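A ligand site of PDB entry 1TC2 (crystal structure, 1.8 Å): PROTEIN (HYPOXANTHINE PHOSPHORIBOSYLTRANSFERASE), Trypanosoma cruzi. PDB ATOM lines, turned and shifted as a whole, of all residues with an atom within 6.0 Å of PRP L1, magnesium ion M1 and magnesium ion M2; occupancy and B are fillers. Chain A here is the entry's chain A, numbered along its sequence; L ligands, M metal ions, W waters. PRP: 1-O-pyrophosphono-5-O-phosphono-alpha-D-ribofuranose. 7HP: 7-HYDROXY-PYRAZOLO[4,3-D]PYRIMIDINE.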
ATOM      1  N   VAL A  50     -27.811 -23.135   7.975  1.00  0.00           N
ATOM      2  CA  VAL A  50     -27.088 -23.985   8.901  1.00  0.00           C
ATOM      3  C   VAL A  50     -25.830 -23.298   9.449  1.00  0.00           C
ATOM      4  O   VAL A  50     -24.843 -23.078   8.732  1.00  0.00           O
ATOM      5  CB  VAL A  50     -26.748 -25.363   8.284  1.00  0.00           C
ATOM      6  CG1 VAL A  50     -26.118 -26.289   9.336  1.00  0.00           C
ATOM      7  CG2 VAL A  50     -28.022 -25.983   7.675  1.00  0.00           C
ATOM      8  N   LEU A  51     -25.844 -22.977  10.739  1.00  0.00           N
ATOM      9  CA  LEU A  51     -24.703 -22.331  11.397  1.00  0.00           C
ATOM     10  C   LEU A  51     -23.512 -23.296  11.501  1.00  0.00           C
ATOM     11  O   LEU A  51     -23.710 -24.515  11.508  1.00  0.00           O
ATOM     12  CB  LEU A  51     -25.121 -21.871  12.796  1.00  0.00           C
ATOM     13  CG  LEU A  51     -26.256 -20.839  12.844  1.00  0.00           C
ATOM     14  CD1 LEU A  51     -26.743 -20.709  14.274  1.00  0.00           C
ATOM     15  CD2 LEU A  51     -25.757 -19.495  12.265  1.00  0.00           C
ATOM     16  N   LYS A  52     -22.281 -22.783  11.588  1.00  0.00           N
ATOM     17  CA  LYS A  52     -21.988 -21.350  11.587  1.00  0.00           C
ATOM     18  C   LYS A  52     -21.606 -20.862  10.168  1.00  0.00           C
ATOM     19  O   LYS A  52     -21.975 -19.770   9.749  1.00  0.00           O
ATOM     20  CB  LYS A  52     -20.796 -21.057  12.522  1.00  0.00           C
ATOM     21  CG  LYS A  52     -21.048 -21.350  13.987  1.00  0.00           C
ATOM     22  CD  LYS A  52     -20.086 -20.573  14.886  1.00  0.00           C
ATOM     23  CE  LYS A  52     -18.753 -21.276  15.084  1.00  0.00           C
ATOM     24  NZ  LYS A  52     -17.740 -20.404  15.773  1.00  0.00           N
ATOM     25  N   GLY A  53     -20.923 -21.737   9.431  1.00  0.00           N
ATOM     26  CA  GLY A  53     -20.437 -21.409   8.099  1.00  0.00           C
ATOM     27  C   GLY A  53     -21.340 -20.721   7.085  1.00  0.00           C
ATOM     28  O   GLY A  53     -20.890 -19.862   6.354  1.00  0.00           O
ATOM     29  N   SER A  54     -22.611 -21.090   7.032  1.00  0.00           N
ATOM     30  CA  SER A  54     -23.488 -20.477   6.045  1.00  0.00           C
ATOM     31  C   SER A  54     -23.924 -19.064   6.365  1.00  0.00           C
ATOM     32  O   SER A  54     -24.582 -18.422   5.543  1.00  0.00           O
ATOM     33  CB  SER A  54     -24.728 -21.341   5.831  1.00  0.00           C
ATOM     34  OG  SER A  54     -25.571 -21.251   6.949  1.00  0.00           O
ATOM     35  N   GLU A 111     -26.563 -24.001   2.952  1.00  0.00           N
ATOM     36  CA  GLU A 111     -25.280 -24.505   3.471  1.00  0.00           C
ATOM     37  C   GLU A 111     -24.127 -23.916   2.696  1.00  0.00           C
ATOM     38  O   GLU A 111     -24.252 -23.568   1.509  1.00  0.00           O
ATOM     39  CB  GLU A 111     -25.206 -26.039   3.358  1.00  0.00           C
ATOM     40  CG  GLU A 111     -25.514 -26.794   4.623  1.00  0.00           C
ATOM     41  CD  GLU A 111     -24.389 -26.722   5.654  1.00  0.00           C
ATOM     42  OE1 GLU A 111     -24.149 -27.744   6.325  1.00  0.00           O
ATOM     43  OE2 GLU A 111     -23.752 -25.656   5.807  1.00  0.00           O
ATOM     44  N   ASP A 112     -22.976 -23.836   3.353  1.00  0.00           N
ATOM     45  CA  ASP A 112     -21.788 -23.292   2.712  1.00  0.00           C
ATOM     46  C   ASP A 112     -21.073 -24.363   1.894  1.00  0.00           C
ATOM     47  O   ASP A 112     -20.598 -24.079   0.792  1.00  0.00           O
ATOM     48  CB  ASP A 112     -20.835 -22.680   3.747  1.00  0.00           C
ATOM     49  CG  ASP A 112     -20.434 -23.656   4.856  1.00  0.00           C
ATOM     50  OD1 ASP A 112     -21.120 -24.689   5.067  1.00  0.00           O
ATOM     51  OD2 ASP A 112     -19.436 -23.371   5.551  1.00  0.00           O
ATOM     52  N   ILE A 113     -21.019 -25.583   2.416  1.00  0.00           N
ATOM     53  CA  ILE A 113     -20.343 -26.667   1.721  1.00  0.00           C
ATOM     54  C   ILE A 113     -20.911 -28.046   2.036  1.00  0.00           C
ATOM     55  O   ILE A 113     -21.428 -28.296   3.137  1.00  0.00           O
ATOM     56  CB  ILE A 113     -18.800 -26.657   1.978  1.00  0.00           C
ATOM     57  CG1 ILE A 113     -18.093 -27.625   1.027  1.00  0.00           C
ATOM     58  CG2 ILE A 113     -18.474 -27.024   3.416  1.00  0.00           C
ATOM     59  CD1 ILE A 113     -16.580 -27.484   0.992  1.00  0.00           C
ATOM     60  N   VAL A 114     -20.914 -28.914   1.028  1.00  0.00           N
ATOM     61  CA  VAL A 114     -21.336 -30.297   1.193  1.00  0.00           C
ATOM     62  C   VAL A 114     -20.198 -31.146   0.667  1.00  0.00           C
ATOM     63  O   VAL A 114     -19.641 -30.891  -0.412  1.00  0.00           O
ATOM     64  CB  VAL A 114     -22.705 -30.610   0.526  1.00  0.00           C
ATOM     65  CG1 VAL A 114     -22.656 -30.420  -0.985  1.00  0.00           C
ATOM     66  CG2 VAL A 114     -23.167 -31.995   0.924  1.00  0.00           C
ATOM     67  N   ASP A 115     -19.771 -32.079   1.506  1.00  0.00           N
ATOM     68  CA  ASP A 115     -18.664 -32.980   1.219  1.00  0.00           C
ATOM     69  C   ASP A 115     -19.158 -34.415   1.420  1.00  0.00           C
ATOM     70  O   ASP A 115     -19.646 -35.042   0.458  1.00  0.00           O
ATOM     71  CB  ASP A 115     -17.518 -32.647   2.174  1.00  0.00           C
ATOM     72  CG  ASP A 115     -16.280 -33.467   1.915  1.00  0.00           C
ATOM     73  OD1 ASP A 115     -16.156 -34.081   0.846  1.00  0.00           O
ATOM     74  OD2 ASP A 115     -15.388 -33.450   2.790  1.00  0.00           O
ATOM     75  N   THR A 116     -19.107 -34.915   2.654  1.00  0.00           N
ATOM     76  CA  THR A 116     -19.562 -36.288   2.919  1.00  0.00           C
ATOM     77  C   THR A 116     -21.067 -36.346   2.879  1.00  0.00           C
ATOM     78  O   THR A 116     -21.652 -37.403   2.594  1.00  0.00           O
ATOM     79  CB  THR A 116     -19.083 -36.794   4.273  1.00  0.00           C
ATOM     80  OG1 THR A 116     -19.788 -36.099   5.323  1.00  0.00           O
ATOM     81  CG2 THR A 116     -17.577 -36.577   4.413  1.00  0.00           C
ATOM     82  N   ALA A 117     -21.682 -35.199   3.137  1.00  0.00           N
ATOM     83  CA  ALA A 117     -23.136 -35.017   3.160  1.00  0.00           C
ATOM     84  C   ALA A 117     -23.856 -35.741   4.294  1.00  0.00           C
ATOM     85  O   ALA A 117     -25.080 -35.718   4.343  1.00  0.00           O
ATOM     86  CB  ALA A 117     -23.746 -35.427   1.818  1.00  0.00           C
ATOM     87  N   LEU A 118     -23.121 -36.334   5.216  1.00  0.00           N
ATOM     88  CA  LEU A 118     -23.784 -37.089   6.281  1.00  0.00           C
ATOM     89  C   LEU A 118     -24.759 -36.270   7.082  1.00  0.00           C
ATOM     90  O   LEU A 118     -25.919 -36.662   7.234  1.00  0.00           O
ATOM     91  CB  LEU A 118     -22.756 -37.747   7.180  1.00  0.00           C
ATOM     92  CG  LEU A 118     -22.001 -38.854   6.461  1.00  0.00           C
ATOM     93  CD1 LEU A 118     -20.815 -39.322   7.290  1.00  0.00           C
ATOM     94  CD2 LEU A 118     -22.989 -39.982   6.179  1.00  0.00           C
ATOM     95  N   THR A 119     -24.322 -35.105   7.559  1.00  0.00           N
ATOM     96  CA  THR A 119     -25.185 -34.224   8.353  1.00  0.00           C
ATOM     97  C   THR A 119     -26.297 -33.607   7.508  1.00  0.00           C
ATOM     98  O   THR A 119     -27.453 -33.620   7.897  1.00  0.00           O
ATOM     99  CB  THR A 119     -24.364 -33.084   9.011  1.00  0.00           C
ATOM    100  OG1 THR A 119     -23.278 -33.649   9.771  1.00  0.00           O
ATOM    101  CG2 THR A 119     -25.251 -32.264   9.956  1.00  0.00           C
ATOM    102  N   LEU A 120     -25.944 -33.074   6.348  1.00  0.00           N
ATOM    103  CA  LEU A 120     -26.940 -32.466   5.491  1.00  0.00           C
ATOM    104  C   LEU A 120     -28.003 -33.484   5.044  1.00  0.00           C
ATOM    105  O   LEU A 120     -29.189 -33.147   4.969  1.00  0.00           O
ATOM    106  CB  LEU A 120     -26.264 -31.823   4.284  1.00  0.00           C
ATOM    107  CG  LEU A 120     -27.215 -31.114   3.335  1.00  0.00           C
ATOM    108  CD1 LEU A 120     -28.109 -30.058   4.052  1.00  0.00           C
ATOM    109  CD2 LEU A 120     -26.386 -30.501   2.242  1.00  0.00           C
ATOM    110  N   GLY A 169     -17.133 -17.495   5.322  1.00  0.00           N
ATOM    111  CA  GLY A 169     -17.903 -18.264   6.282  1.00  0.00           C
ATOM    112  C   GLY A 169     -17.239 -19.561   6.684  1.00  0.00           C
ATOM    113  O   GLY A 169     -17.435 -20.044   7.792  1.00  0.00           O
ATOM    114  N   LEU A 170     -16.460 -20.132   5.776  1.00  0.00           N
ATOM    115  CA  LEU A 170     -15.745 -21.391   5.992  1.00  0.00           C
ATOM    116  C   LEU A 170     -14.494 -21.242   6.840  1.00  0.00           C
ATOM    117  O   LEU A 170     -13.604 -20.458   6.521  1.00  0.00           O
ATOM    118  CB  LEU A 170     -15.331 -21.977   4.641  1.00  0.00           C
ATOM    119  CG  LEU A 170     -16.491 -22.423   3.775  1.00  0.00           C
ATOM    120  CD1 LEU A 170     -16.155 -22.145   2.347  1.00  0.00           C
ATOM    121  CD2 LEU A 170     -16.768 -23.902   3.993  1.00  0.00           C
ATOM    122  N   ASP A 171     -14.327 -22.136   7.804  1.00  0.00           N
ATOM    123  CA  ASP A 171     -13.175 -22.057   8.679  1.00  0.00           C
ATOM    124  C   ASP A 171     -12.279 -23.273   8.739  1.00  0.00           C
ATOM    125  O   ASP A 171     -12.618 -24.375   8.295  1.00  0.00           O
ATOM    126  CB  ASP A 171     -13.649 -21.871  10.111  1.00  0.00           C
ATOM    127  CG  ASP A 171     -14.264 -23.144  10.684  1.00  0.00           C
ATOM    128  OD1 ASP A 171     -15.275 -23.638  10.112  1.00  0.00           O
ATOM    129  OD2 ASP A 171     -13.722 -23.666  11.686  1.00  0.00           O
ATOM    130  N   TYR A 172     -11.174 -23.055   9.436  1.00  0.00           N
ATOM    131  CA  TYR A 172     -10.234 -24.090   9.792  1.00  0.00           C
ATOM    132  C   TYR A 172      -9.977 -23.701  11.250  1.00  0.00           C
ATOM    133  O   TYR A 172      -9.506 -22.596  11.523  1.00  0.00           O
ATOM    134  CB  TYR A 172      -8.912 -24.028   9.040  1.00  0.00           C
ATOM    135  CG  TYR A 172      -7.879 -24.833   9.803  1.00  0.00           C
ATOM    136  CD1 TYR A 172      -8.099 -26.183  10.091  1.00  0.00           C
ATOM    137  CD2 TYR A 172      -6.747 -24.224  10.347  1.00  0.00           C
ATOM    138  CE1 TYR A 172      -7.222 -26.900  10.916  1.00  0.00           C
ATOM    139  CE2 TYR A 172      -5.874 -24.925  11.171  1.00  0.00           C
ATOM    140  CZ  TYR A 172      -6.120 -26.256  11.456  1.00  0.00           C
ATOM    141  OH  TYR A 172      -5.249 -26.939  12.279  1.00  0.00           O
ATOM    142  N   ARG A 177     -13.014 -17.396   8.837  1.00  0.00           N
ATOM    143  CA  ARG A 177     -14.380 -17.314   8.339  1.00  0.00           C
ATOM    144  C   ARG A 177     -14.678 -15.964   7.697  1.00  0.00           C
ATOM    145  O   ARG A 177     -15.502 -15.859   6.789  1.00  0.00           O
ATOM    146  CB  ARG A 177     -15.409 -17.508   9.453  1.00  0.00           C
ATOM    147  CG  ARG A 177     -15.314 -18.776  10.246  1.00  0.00           C
ATOM    148  CD  ARG A 177     -16.634 -18.999  10.981  1.00  0.00           C
ATOM    149  NE  ARG A 177     -16.555 -20.155  11.862  1.00  0.00           N
ATOM    150  CZ  ARG A 177     -16.909 -21.393  11.514  1.00  0.00           C
ATOM    151  NH1 ARG A 177     -17.376 -21.645  10.293  1.00  0.00           N
ATOM    152  NH2 ARG A 177     -16.711 -22.380  12.372  1.00  0.00           N
HETATM  153  C1  PRP L   1     -18.863 -27.919   7.957  1.00  0.00           C
HETATM  154  C2  PRP L   1     -19.461 -27.069   6.850  1.00  0.00           C
HETATM  155  C3  PRP L   1     -20.726 -27.912   6.537  1.00  0.00           C
HETATM  156  C4  PRP L   1     -20.170 -29.353   6.710  1.00  0.00           C
HETATM  157  C5  PRP L   1     -19.692 -29.854   5.319  1.00  0.00           C
HETATM  158  O1  PRP L   1     -19.516 -27.578   9.216  1.00  0.00           O
HETATM  159  O2  PRP L   1     -19.740 -25.716   7.392  1.00  0.00           O
HETATM  160  O3  PRP L   1     -21.805 -27.793   7.451  1.00  0.00           O
HETATM  161  O4  PRP L   1     -19.070 -29.283   7.649  1.00  0.00           O
HETATM  162  O5  PRP L   1     -19.047 -31.155   5.294  1.00  0.00           O
HETATM  163  P   PRP L   1     -19.812 -32.662   5.290  1.00  0.00           P
HETATM  164  O1P PRP L   1     -20.729 -32.686   4.098  1.00  0.00           O
HETATM  165  O2P PRP L   1     -20.593 -32.676   6.553  1.00  0.00           O
HETATM  166  O3P PRP L   1     -18.639 -33.597   5.259  1.00  0.00           O
HETATM  167  PA  PRP L   1     -18.710 -27.611  10.641  1.00  0.00           P
HETATM  168  O1A PRP L   1     -18.844 -28.921  11.279  1.00  0.00           O
HETATM  169  O2A PRP L   1     -17.303 -27.324  10.317  1.00  0.00           O
HETATM  170  O3A PRP L   1     -19.393 -26.489  11.370  1.00  0.00           O
HETATM  171  PB  PRP L   1     -19.280 -25.005  11.101  1.00  0.00           P
HETATM  172  O1B PRP L   1     -17.874 -24.601  10.765  1.00  0.00           O
HETATM  173  O2B PRP L   1     -19.716 -24.282  12.275  1.00  0.00           O
HETATM  174  O3B PRP L   1     -20.211 -24.606  10.026  1.00  0.00           O
HETATM  175  C9  7HP L   2     -15.976 -29.002   5.714  1.00  0.00           C
HETATM  176  C4  7HP L   2     -15.109 -27.952   5.439  1.00  0.00           C
HETATM  177  N3  7HP L   2     -14.974 -26.804   6.148  1.00  0.00           N
HETATM  178  C2  7HP L   2     -14.071 -25.969   5.539  1.00  0.00           C
HETATM  179  N1  7HP L   2     -13.383 -26.299   4.389  1.00  0.00           N
HETATM  180  C6  7HP L   2     -13.511 -27.467   3.698  1.00  0.00           C
HETATM  181  O6  7HP L   2     -12.802 -27.704   2.733  1.00  0.00           O
HETATM  182  C5  7HP L   2     -14.432 -28.308   4.286  1.00  0.00           C
HETATM  183  N7  7HP L   2     -14.879 -29.548   3.905  1.00  0.00           N
HETATM  184  N8  7HP L   2     -15.771 -29.888   4.779  1.00  0.00           N
HETATM  185 MG    MG M   1     -21.390 -25.959   8.754  1.00  0.00          MG
HETATM  186 MG    MG M   2     -16.062 -25.638  10.190  1.00  0.00          MG
HETATM  187  O   HOH W   1     -14.992 -29.358   9.258  1.00  0.00           O
HETATM  188  O   HOH W   2     -21.288 -25.561  13.937  1.00  0.00           O
HETATM  189  O   HOH W   3     -21.551 -34.663   7.748  1.00  0.00           O
HETATM  190  O   HOH W   4     -22.220 -26.759  10.407  1.00  0.00           O
HETATM  191  O   HOH W   5     -16.195 -32.858   5.383  1.00  0.00           O
HETATM  192  O   HOH W   6     -17.868 -24.705  14.355  1.00  0.00           O
HETATM  193  O   HOH W   7     -15.644 -25.747  12.268  1.00  0.00           O
HETATM  194  O   HOH W   8     -21.764 -28.922  12.075  1.00  0.00           O
HETATM  195  O   HOH W   9     -23.519 -29.220   9.982  1.00  0.00           O
HETATM  196  O   HOH W  10     -16.560 -25.365   8.252  1.00  0.00           O
HETATM  197  O   HOH W  11     -22.659 -24.666   8.005  1.00  0.00           O
HETATM  198  O   HOH W  12     -14.228 -26.552   9.612  1.00  0.00           O
HETATM  199  O   HOH W  13     -23.149 -32.336   5.673  1.00  0.00           O
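An oxygen (O1P) of PRP L1 is in hydrogen-bond range of the backbone NH (N) of Ala 117.
The side-chain carboxylate (OE1) of Glu 111 lies close to an oxygen (O3) of PRP L1 (2.6 Å).
The backbone NH of Gly 53 lies close to an oxygen (O3B) of PRP L1.
N of Lys 52 lies within hydrogen-bond range of O2B of PRP L1, 3.0 Å away.
O3P of PRP L1 sits at hydrogen-bond distance from OG1 of Thr 116 (2.8 Å).
An oxygen (O2B) of PRP L1 is in salt-bridge range of the guanidinium group of Arg 177 (3.6 Å).
The side-chain carboxylate (OD1) of Asp 112 sits close to an oxygen (O2) of PRP L1 (2.9 Å).
An oxygen (O1P) of PRP L1 sits at hydrogen-bond distance from the backbone NH (N) of Asp 115, at 2.8 Å.
An oxygen (O3P) of PRP L1 sits at hydrogen-bond distance from the backbone NH of Thr 116.
Merely in contact with PRP L1: Ile 113, Val 114 and Leu 51.
Hydrophobic or aromatic side chains within 4 Å of PRP L1: Ile 113.
Of the 20 residues printed, 12 come within 4 Å of PRP L1.
Along chain A the residues within 4 Å of PRP L1 span positions 51 to 177.
Residues that only touch magnesium ion M2: Arg 177.
Within 4 Å of magnesium ion M2: Asp 171 and Arg 177.
The nearest printed residue that does not touch magnesium ion M2 is Tyr 172 (5.6 Å).
Magnesium ion M2 is bound by water W10 (2.0 Å), O2A of PRP L1 (2.1 Å), water W7 (2.1 Å), water W12 (2.1 Å), OD1 of Asp 171 (2.2 Å) and O1B of PRP L1 (2.2 Å).
Merely in contact with magnesium ion M1: Leu 51, Glu 111 and Asp 112.
Of the 20 residues printed, 3 come within 4 Å of magnesium ion M1.
Along chain A the residues within 4 Å of magnesium ion M1 span positions 51 to 112.
The nearest printed residue that does not touch magnesium ion M1 is Gly 53 (4.3 Å).
Magnesium ion M1 is bound by water W11, at 2.0 Å.
Water W4 is bound to magnesium ion M1.
O2 of PRP L1 binds magnesium ion M1 (2.2 Å).
O3B of PRP L1 binds magnesium ion M1, 2.2 Å away.
O3 of PRP L1 binds magnesium ion M1 (2.3 Å).
O1 of PRP L1 binds magnesium ion M1, at 2.5 Å.
OG1 of Thr 116 sits close to N of Leu 118 (3.3 Å).
The side-chain carboxylate (OD2) of Asp 171 is in salt-bridge range of the guanidinium group (NH2) of Arg 177, 3.3 Å away.
The backbone carbonyl oxygen of Arg 177 sits at hydrogen-bond distance from the backbone NH of Gly 169 (2.7 Å).
Water W4 bridges O of Leu 51 (2.9 Å) and O3A of PRP L1 (3.0 Å).
Water W3 lies within hydrogen-bond range of an oxygen (O2P) of PRP L1 (2.5 Å), the backbone NH (N) of Thr 119 (2.8 Å), the side-chain hydroxyl (OG1) of Thr 116 (3.3 Å) and the backbone NH (N) of Leu 118 (3.4 Å).
Water W5 lies within hydrogen-bond range of an oxygen (O3P) of PRP L1 (2.6 Å), the side-chain carboxylate of Asp 115 (2.8 Å) and a nitrogen (N8) of 7HP L2 (3.1 Å).
Water W13 bridges O2P of PRP L1 and N of Leu 120.
Water W6 bridges O2B of PRP L1 (2.8 Å) and NH2 of Arg 177 (3.3 Å).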
